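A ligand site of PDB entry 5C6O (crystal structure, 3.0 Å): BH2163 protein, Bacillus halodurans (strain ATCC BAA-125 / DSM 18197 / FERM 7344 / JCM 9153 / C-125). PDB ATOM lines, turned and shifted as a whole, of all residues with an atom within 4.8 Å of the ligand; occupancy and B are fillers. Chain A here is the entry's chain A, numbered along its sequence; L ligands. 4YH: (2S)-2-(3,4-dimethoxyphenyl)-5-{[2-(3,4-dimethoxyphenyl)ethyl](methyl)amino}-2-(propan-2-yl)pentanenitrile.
O20 of the ligand is in hydrogen-bond range of ND2 of Asn 37 (2.4 Å). An oxygen (O23) of the ligand lies within hydrogen-bond range of the side-chain amide nitrogen of Gln 252.
The guanidinium group (NE) of Arg 283 sits close to the side-chain amide oxygen (OD1) of Asn 37 (2.9 Å). OE1 of Gln 252 sits close to SD of Met 64 (3.3 Å).
Met 33 touches the ligand (CE to C29, 3.4 Å). CD2 of Tyr 36 touches O24 of the ligand, 3.5 Å away. Phe 60 touches the ligand (CE1 to C12, 3.8 Å). Met 63 touches the ligand. Met 64 touches the ligand (N to C27, 3.8 Å). SD of Met 67 touches C11 of the ligand, 2.9 Å away. CZ of Phe 150 touches N8 of the ligand (3.3 Å). Phe 154 touches the ligand. Hydrophobic or aromatic side chains within 4 Å of the ligand: Met 33, Tyr 36, Phe 60, Met 63, Met 64, Met 67, Phe 150 and Phe 154. The nearest printed residue that does not touch the ligand is Arg 283 (4.02 Å).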
ATOM      1  N   MET A  33       4.660  26.018 -30.112  1.00  0.00           N
ATOM      2  CA  MET A  33       5.051  25.593 -28.791  1.00  0.00           C
ATOM      3  C   MET A  33       4.073  26.161 -27.783  1.00  0.00           C
ATOM      4  O   MET A  33       3.672  25.477 -26.862  1.00  0.00           O
ATOM      5  CB  MET A  33       6.478  26.015 -28.498  1.00  0.00           C
ATOM      6  CG  MET A  33       7.233  25.012 -27.639  1.00  0.00           C
ATOM      7  SD  MET A  33       8.619  25.781 -26.758  1.00  0.00           S
ATOM      8  CE  MET A  33       7.798  27.184 -25.969  1.00  0.00           C
ATOM      9  N   ALA A  34       3.668  27.400 -27.987  1.00  0.00           N
ATOM     10  CA  ALA A  34       2.656  27.990 -27.138  1.00  0.00           C
ATOM     11  C   ALA A  34       1.425  27.061 -27.020  1.00  0.00           C
ATOM     12  O   ALA A  34       0.894  26.867 -25.926  1.00  0.00           O
ATOM     13  CB  ALA A  34       2.290  29.378 -27.632  1.00  0.00           C
ATOM     14  N   TYR A  36       1.582  23.650 -27.243  1.00  0.00           N
ATOM     15  CA  TYR A  36       2.040  22.657 -26.267  1.00  0.00           C
ATOM     16  C   TYR A  36       1.803  23.064 -24.819  1.00  0.00           C
ATOM     17  O   TYR A  36       1.410  22.241 -24.017  1.00  0.00           O
ATOM     18  CB  TYR A  36       3.506  22.287 -26.429  1.00  0.00           C
ATOM     19  CG  TYR A  36       4.109  21.777 -25.110  1.00  0.00           C
ATOM     20  CD1 TYR A  36       4.158  20.416 -24.831  1.00  0.00           C
ATOM     21  CD2 TYR A  36       4.619  22.660 -24.143  1.00  0.00           C
ATOM     22  CE1 TYR A  36       4.685  19.952 -23.638  1.00  0.00           C
ATOM     23  CE2 TYR A  36       5.159  22.196 -22.951  1.00  0.00           C
ATOM     24  CZ  TYR A  36       5.193  20.837 -22.699  1.00  0.00           C
ATOM     25  OH  TYR A  36       5.719  20.373 -21.506  1.00  0.00           O
ATOM     26  N   ASN A  37       2.086  24.299 -24.459  1.00  0.00           N
ATOM     27  CA  ASN A  37       1.743  24.751 -23.148  1.00  0.00           C
ATOM     28  C   ASN A  37       0.312  24.351 -22.897  1.00  0.00           C
ATOM     29  O   ASN A  37       0.042  23.200 -22.504  1.00  0.00           O
ATOM     30  CB  ASN A  37       1.808  26.268 -23.067  1.00  0.00           C
ATOM     31  CG  ASN A  37       1.969  26.744 -21.637  1.00  0.00           C
ATOM     32  OD1 ASN A  37       1.646  27.890 -21.308  1.00  0.00           O
ATOM     33  ND2 ASN A  37       2.474  25.865 -20.776  1.00  0.00           N
ATOM     34  N   VAL A  56       4.302  23.287 -10.896  1.00  0.00           N
ATOM     35  CA  VAL A  56       4.616  23.954 -12.146  1.00  0.00           C
ATOM     36  C   VAL A  56       5.001  25.426 -12.009  1.00  0.00           C
ATOM     37  O   VAL A  56       6.144  25.822 -12.308  1.00  0.00           O
ATOM     38  CB  VAL A  56       3.380  23.904 -13.070  1.00  0.00           C
ATOM     39  CG1 VAL A  56       3.556  24.822 -14.309  1.00  0.00           C
ATOM     40  CG2 VAL A  56       3.069  22.447 -13.446  1.00  0.00           C
ATOM     41  N   PHE A  60       8.276  27.168 -12.135  1.00  0.00           N
ATOM     42  CA  PHE A  60       8.644  27.933 -13.323  1.00  0.00           C
ATOM     43  C   PHE A  60       9.913  28.801 -13.180  1.00  0.00           C
ATOM     44  O   PHE A  60      10.944  28.482 -13.787  1.00  0.00           O
ATOM     45  CB  PHE A  60       7.452  28.763 -13.814  1.00  0.00           C
ATOM     46  CG  PHE A  60       7.651  29.333 -15.191  1.00  0.00           C
ATOM     47  CD1 PHE A  60       7.127  28.684 -16.307  1.00  0.00           C
ATOM     48  CD2 PHE A  60       8.352  30.534 -15.379  1.00  0.00           C
ATOM     49  CE1 PHE A  60       7.301  29.212 -17.579  1.00  0.00           C
ATOM     50  CE2 PHE A  60       8.527  31.053 -16.652  1.00  0.00           C
ATOM     51  CZ  PHE A  60       8.004  30.393 -17.755  1.00  0.00           C
ATOM     52  N   MET A  63      13.324  27.426 -13.808  1.00  0.00           N
ATOM     53  CA  MET A  63      13.718  27.102 -15.162  1.00  0.00           C
ATOM     54  C   MET A  63      14.169  28.384 -15.873  1.00  0.00           C
ATOM     55  O   MET A  63      15.152  28.415 -16.603  1.00  0.00           O
ATOM     56  CB  MET A  63      12.546  26.538 -15.922  1.00  0.00           C
ATOM     57  CG  MET A  63      11.949  25.306 -15.317  1.00  0.00           C
ATOM     58  SD  MET A  63      10.693  24.731 -16.455  1.00  0.00           S
ATOM     59  CE  MET A  63      11.735  24.062 -17.754  1.00  0.00           C
ATOM     60  N   MET A  64      13.431  29.461 -15.645  1.00  0.00           N
ATOM     61  CA  MET A  64      13.763  30.715 -16.248  1.00  0.00           C
ATOM     62  C   MET A  64      15.140  31.190 -15.804  1.00  0.00           C
ATOM     63  O   MET A  64      15.819  31.847 -16.557  1.00  0.00           O
ATOM     64  CB  MET A  64      12.711  31.758 -15.884  1.00  0.00           C
ATOM     65  CG  MET A  64      12.972  33.126 -16.465  1.00  0.00           C
ATOM     66  SD  MET A  64      12.632  33.202 -18.233  1.00  0.00           S
ATOM     67  CE  MET A  64      10.870  33.485 -18.219  1.00  0.00           C
ATOM     68  N   MET A  67      17.600  29.043 -18.174  1.00  0.00           N
ATOM     69  CA  MET A  67      17.450  29.519 -19.546  1.00  0.00           C
ATOM     70  C   MET A  67      17.800  30.993 -19.783  1.00  0.00           C
ATOM     71  O   MET A  67      18.315  31.335 -20.856  1.00  0.00           O
ATOM     72  CB  MET A  67      16.052  29.197 -20.039  1.00  0.00           C
ATOM     73  CG  MET A  67      15.858  29.507 -21.499  1.00  0.00           C
ATOM     74  SD  MET A  67      14.285  30.360 -21.637  1.00  0.00           S
ATOM     75  CE  MET A  67      14.381  31.543 -20.291  1.00  0.00           C
ATOM     76  N   TYR A 139       8.397  18.155 -10.630  1.00  0.00           N
ATOM     77  CA  TYR A 139       8.502  18.877 -11.866  1.00  0.00           C
ATOM     78  C   TYR A 139       9.950  19.247 -12.106  1.00  0.00           C
ATOM     79  O   TYR A 139      10.470  19.038 -13.190  1.00  0.00           O
ATOM     80  CB  TYR A 139       7.651  20.126 -11.842  1.00  0.00           C
ATOM     81  CG  TYR A 139       7.506  20.751 -13.201  1.00  0.00           C
ATOM     82  CD1 TYR A 139       7.168  19.984 -14.321  1.00  0.00           C
ATOM     83  CD2 TYR A 139       7.698  22.119 -13.378  1.00  0.00           C
ATOM     84  CE1 TYR A 139       7.034  20.552 -15.587  1.00  0.00           C
ATOM     85  CE2 TYR A 139       7.555  22.715 -14.633  1.00  0.00           C
ATOM     86  CZ  TYR A 139       7.227  21.927 -15.735  1.00  0.00           C
ATOM     87  OH  TYR A 139       7.079  22.521 -16.968  1.00  0.00           O
ATOM     88  N   PHE A 150      18.384  21.098 -22.668  1.00  0.00           N
ATOM     89  CA  PHE A 150      17.550  22.245 -22.512  1.00  0.00           C
ATOM     90  C   PHE A 150      18.252  23.496 -23.024  1.00  0.00           C
ATOM     91  O   PHE A 150      17.712  24.201 -23.875  1.00  0.00           O
ATOM     92  CB  PHE A 150      17.195  22.350 -21.037  1.00  0.00           C
ATOM     93  CG  PHE A 150      16.093  23.307 -20.755  1.00  0.00           C
ATOM     94  CD1 PHE A 150      14.789  22.851 -20.576  1.00  0.00           C
ATOM     95  CD2 PHE A 150      16.348  24.665 -20.667  1.00  0.00           C
ATOM     96  CE1 PHE A 150      13.767  23.746 -20.327  1.00  0.00           C
ATOM     97  CE2 PHE A 150      15.326  25.560 -20.418  1.00  0.00           C
ATOM     98  CZ  PHE A 150      14.036  25.105 -20.240  1.00  0.00           C
ATOM     99  N   PHE A 154      18.095  26.092 -26.942  1.00  0.00           N
ATOM    100  CA  PHE A 154      17.694  27.511 -27.010  1.00  0.00           C
ATOM    101  C   PHE A 154      18.873  28.307 -27.485  1.00  0.00           C
ATOM    102  O   PHE A 154      18.720  29.323 -28.155  1.00  0.00           O
ATOM    103  CB  PHE A 154      17.218  28.062 -25.666  1.00  0.00           C
ATOM    104  CG  PHE A 154      15.940  27.459 -25.181  1.00  0.00           C
ATOM    105  CD1 PHE A 154      15.874  26.908 -23.913  1.00  0.00           C
ATOM    106  CD2 PHE A 154      14.810  27.417 -26.000  1.00  0.00           C
ATOM    107  CE1 PHE A 154      14.705  26.336 -23.463  1.00  0.00           C
ATOM    108  CE2 PHE A 154      13.635  26.834 -25.543  1.00  0.00           C
ATOM    109  CZ  PHE A 154      13.583  26.293 -24.275  1.00  0.00           C
ATOM    110  N   GLN A 252      15.335  38.840 -18.247  1.00  0.00           N
ATOM    111  CA  GLN A 252      14.666  37.714 -17.648  1.00  0.00           C
ATOM    112  C   GLN A 252      14.711  37.822 -16.134  1.00  0.00           C
ATOM    113  O   GLN A 252      13.708  38.181 -15.497  1.00  0.00           O
ATOM    114  CB  GLN A 252      15.284  36.390 -18.123  1.00  0.00           C
ATOM    115  CG  GLN A 252      15.076  36.107 -19.604  1.00  0.00           C
ATOM    116  CD  GLN A 252      13.688  36.482 -20.117  1.00  0.00           C
ATOM    117  OE1 GLN A 252      12.675  36.233 -19.446  1.00  0.00           O
ATOM    118  NE2 GLN A 252      13.641  37.090 -21.315  1.00  0.00           N
ATOM    119  N   ARG A 283       0.286  33.239 -20.597  1.00  0.00           N
ATOM    120  CA  ARG A 283       0.325  32.792 -21.970  1.00  0.00           C
ATOM    121  C   ARG A 283      -0.773  33.421 -22.847  1.00  0.00           C
ATOM    122  O   ARG A 283      -0.902  33.035 -24.023  1.00  0.00           O
ATOM    123  CB  ARG A 283       0.306  31.266 -22.026  1.00  0.00           C
ATOM    124  CG  ARG A 283       1.165  30.594 -20.962  1.00  0.00           C
ATOM    125  CD  ARG A 283       0.412  30.454 -19.640  1.00  0.00           C
ATOM    126  NE  ARG A 283       0.881  29.318 -18.848  1.00  0.00           N
ATOM    127  CZ  ARG A 283       0.116  28.297 -18.476  1.00  0.00           C
ATOM    128  NH1 ARG A 283      -1.177  28.259 -18.796  1.00  0.00           N
ATOM    129  NH2 ARG A 283       0.653  27.313 -17.762  1.00  0.00           N
ATOM    130  N   MET A 286       2.009  36.560 -23.335  1.00  0.00           N
ATOM    131  CA  MET A 286       2.971  35.966 -24.295  1.00  0.00           C
ATOM    132  C   MET A 286       2.375  35.585 -25.647  1.00  0.00           C
ATOM    133  O   MET A 286       2.968  35.841 -26.704  1.00  0.00           O
ATOM    134  CB  MET A 286       3.633  34.709 -23.699  1.00  0.00           C
ATOM    135  CG  MET A 286       4.786  34.167 -24.527  1.00  0.00           C
ATOM    136  SD  MET A 286       4.705  32.394 -24.899  1.00  0.00           S
ATOM    137  CE  MET A 286       3.768  32.390 -26.448  1.00  0.00           C
ATOM    138  N   MET A 293       7.056  39.758 -30.825  1.00  0.00           N
ATOM    139  CA  MET A 293       8.264  38.969 -30.660  1.00  0.00           C
ATOM    140  C   MET A 293       8.809  38.451 -31.993  1.00  0.00           C
ATOM    141  O   MET A 293      10.007  38.589 -32.296  1.00  0.00           O
ATOM    142  CB  MET A 293       7.964  37.797 -29.724  1.00  0.00           C
ATOM    143  CG  MET A 293       7.863  38.184 -28.281  1.00  0.00           C
ATOM    144  SD  MET A 293       9.485  38.435 -27.513  1.00  0.00           S
ATOM    145  CE  MET A 293       9.376  40.151 -26.982  1.00  0.00           C
HETATM  146  C30 4YH L   1       9.787  35.463 -21.325  1.00  0.00           C
HETATM  147  O19 4YH L   1      10.058  35.187 -22.751  1.00  0.00           O
HETATM  148  C6  4YH L   1      10.898  34.132 -22.928  1.00  0.00           C
HETATM  149  C5  4YH L   1      10.439  32.808 -22.869  1.00  0.00           C
HETATM  150  C9  4YH L   1      12.253  34.398 -23.184  1.00  0.00           C
HETATM  151  O23 4YH L   1      12.708  35.691 -23.239  1.00  0.00           O
HETATM  152  C32 4YH L   1      12.095  36.590 -24.402  1.00  0.00           C
HETATM  153  C13 4YH L   1      13.137  33.326 -23.366  1.00  0.00           C
HETATM  154  C11 4YH L   1      12.656  32.010 -23.297  1.00  0.00           C
HETATM  155  C2  4YH L   1      11.303  31.715 -23.044  1.00  0.00           C
HETATM  156  C1  4YH L   1      10.753  30.373 -22.972  1.00  0.00           C
HETATM  157  C15 4YH L   1      10.985  29.573 -24.311  1.00  0.00           C
HETATM  158  C29 4YH L   1      10.618  28.072 -24.224  1.00  0.00           C
HETATM  159  C28 4YH L   1      12.391  29.763 -24.919  1.00  0.00           C
HETATM  160  C3  4YH L   1       9.318  30.559 -22.864  1.00  0.00           C
HETATM  161  N4  4YH L   1       8.134  30.685 -22.802  1.00  0.00           N
HETATM  162  C22 4YH L   1      11.102  29.690 -21.605  1.00  0.00           C
HETATM  163  C26 4YH L   1      12.101  28.507 -21.585  1.00  0.00           C
HETATM  164  C25 4YH L   1      11.410  27.205 -21.164  1.00  0.00           C
HETATM  165  N8  4YH L   1      11.329  26.958 -19.705  1.00  0.00           N
HETATM  166  C27 4YH L   1      12.065  27.928 -18.863  1.00  0.00           C
HETATM  167  C16 4YH L   1       9.904  26.879 -19.335  1.00  0.00           C
HETATM  168  C21 4YH L   1       9.328  25.475 -19.601  1.00  0.00           C
HETATM  169  C17 4YH L   1       8.141  25.540 -20.306  1.00  0.00           C
HETATM  170  C12 4YH L   1       6.982  26.041 -19.702  1.00  0.00           C
HETATM  171  C18 4YH L   1       8.121  25.083 -21.624  1.00  0.00           C
HETATM  172  C14 4YH L   1       6.934  25.139 -22.344  1.00  0.00           C
HETATM  173  C10 4YH L   1       5.774  25.652 -21.753  1.00  0.00           C
HETATM  174  O24 4YH L   1       4.622  25.709 -22.469  1.00  0.00           O
HETATM  175  C33 4YH L   1       4.889  26.335 -23.739  1.00  0.00           C
HETATM  176  C7  4YH L   1       5.780  26.106 -20.420  1.00  0.00           C
HETATM  177  O20 4YH L   1       4.619  26.592 -19.874  1.00  0.00           O
HETATM  178  C31 4YH L   1       4.555  26.577 -18.418  1.00  0.00           C
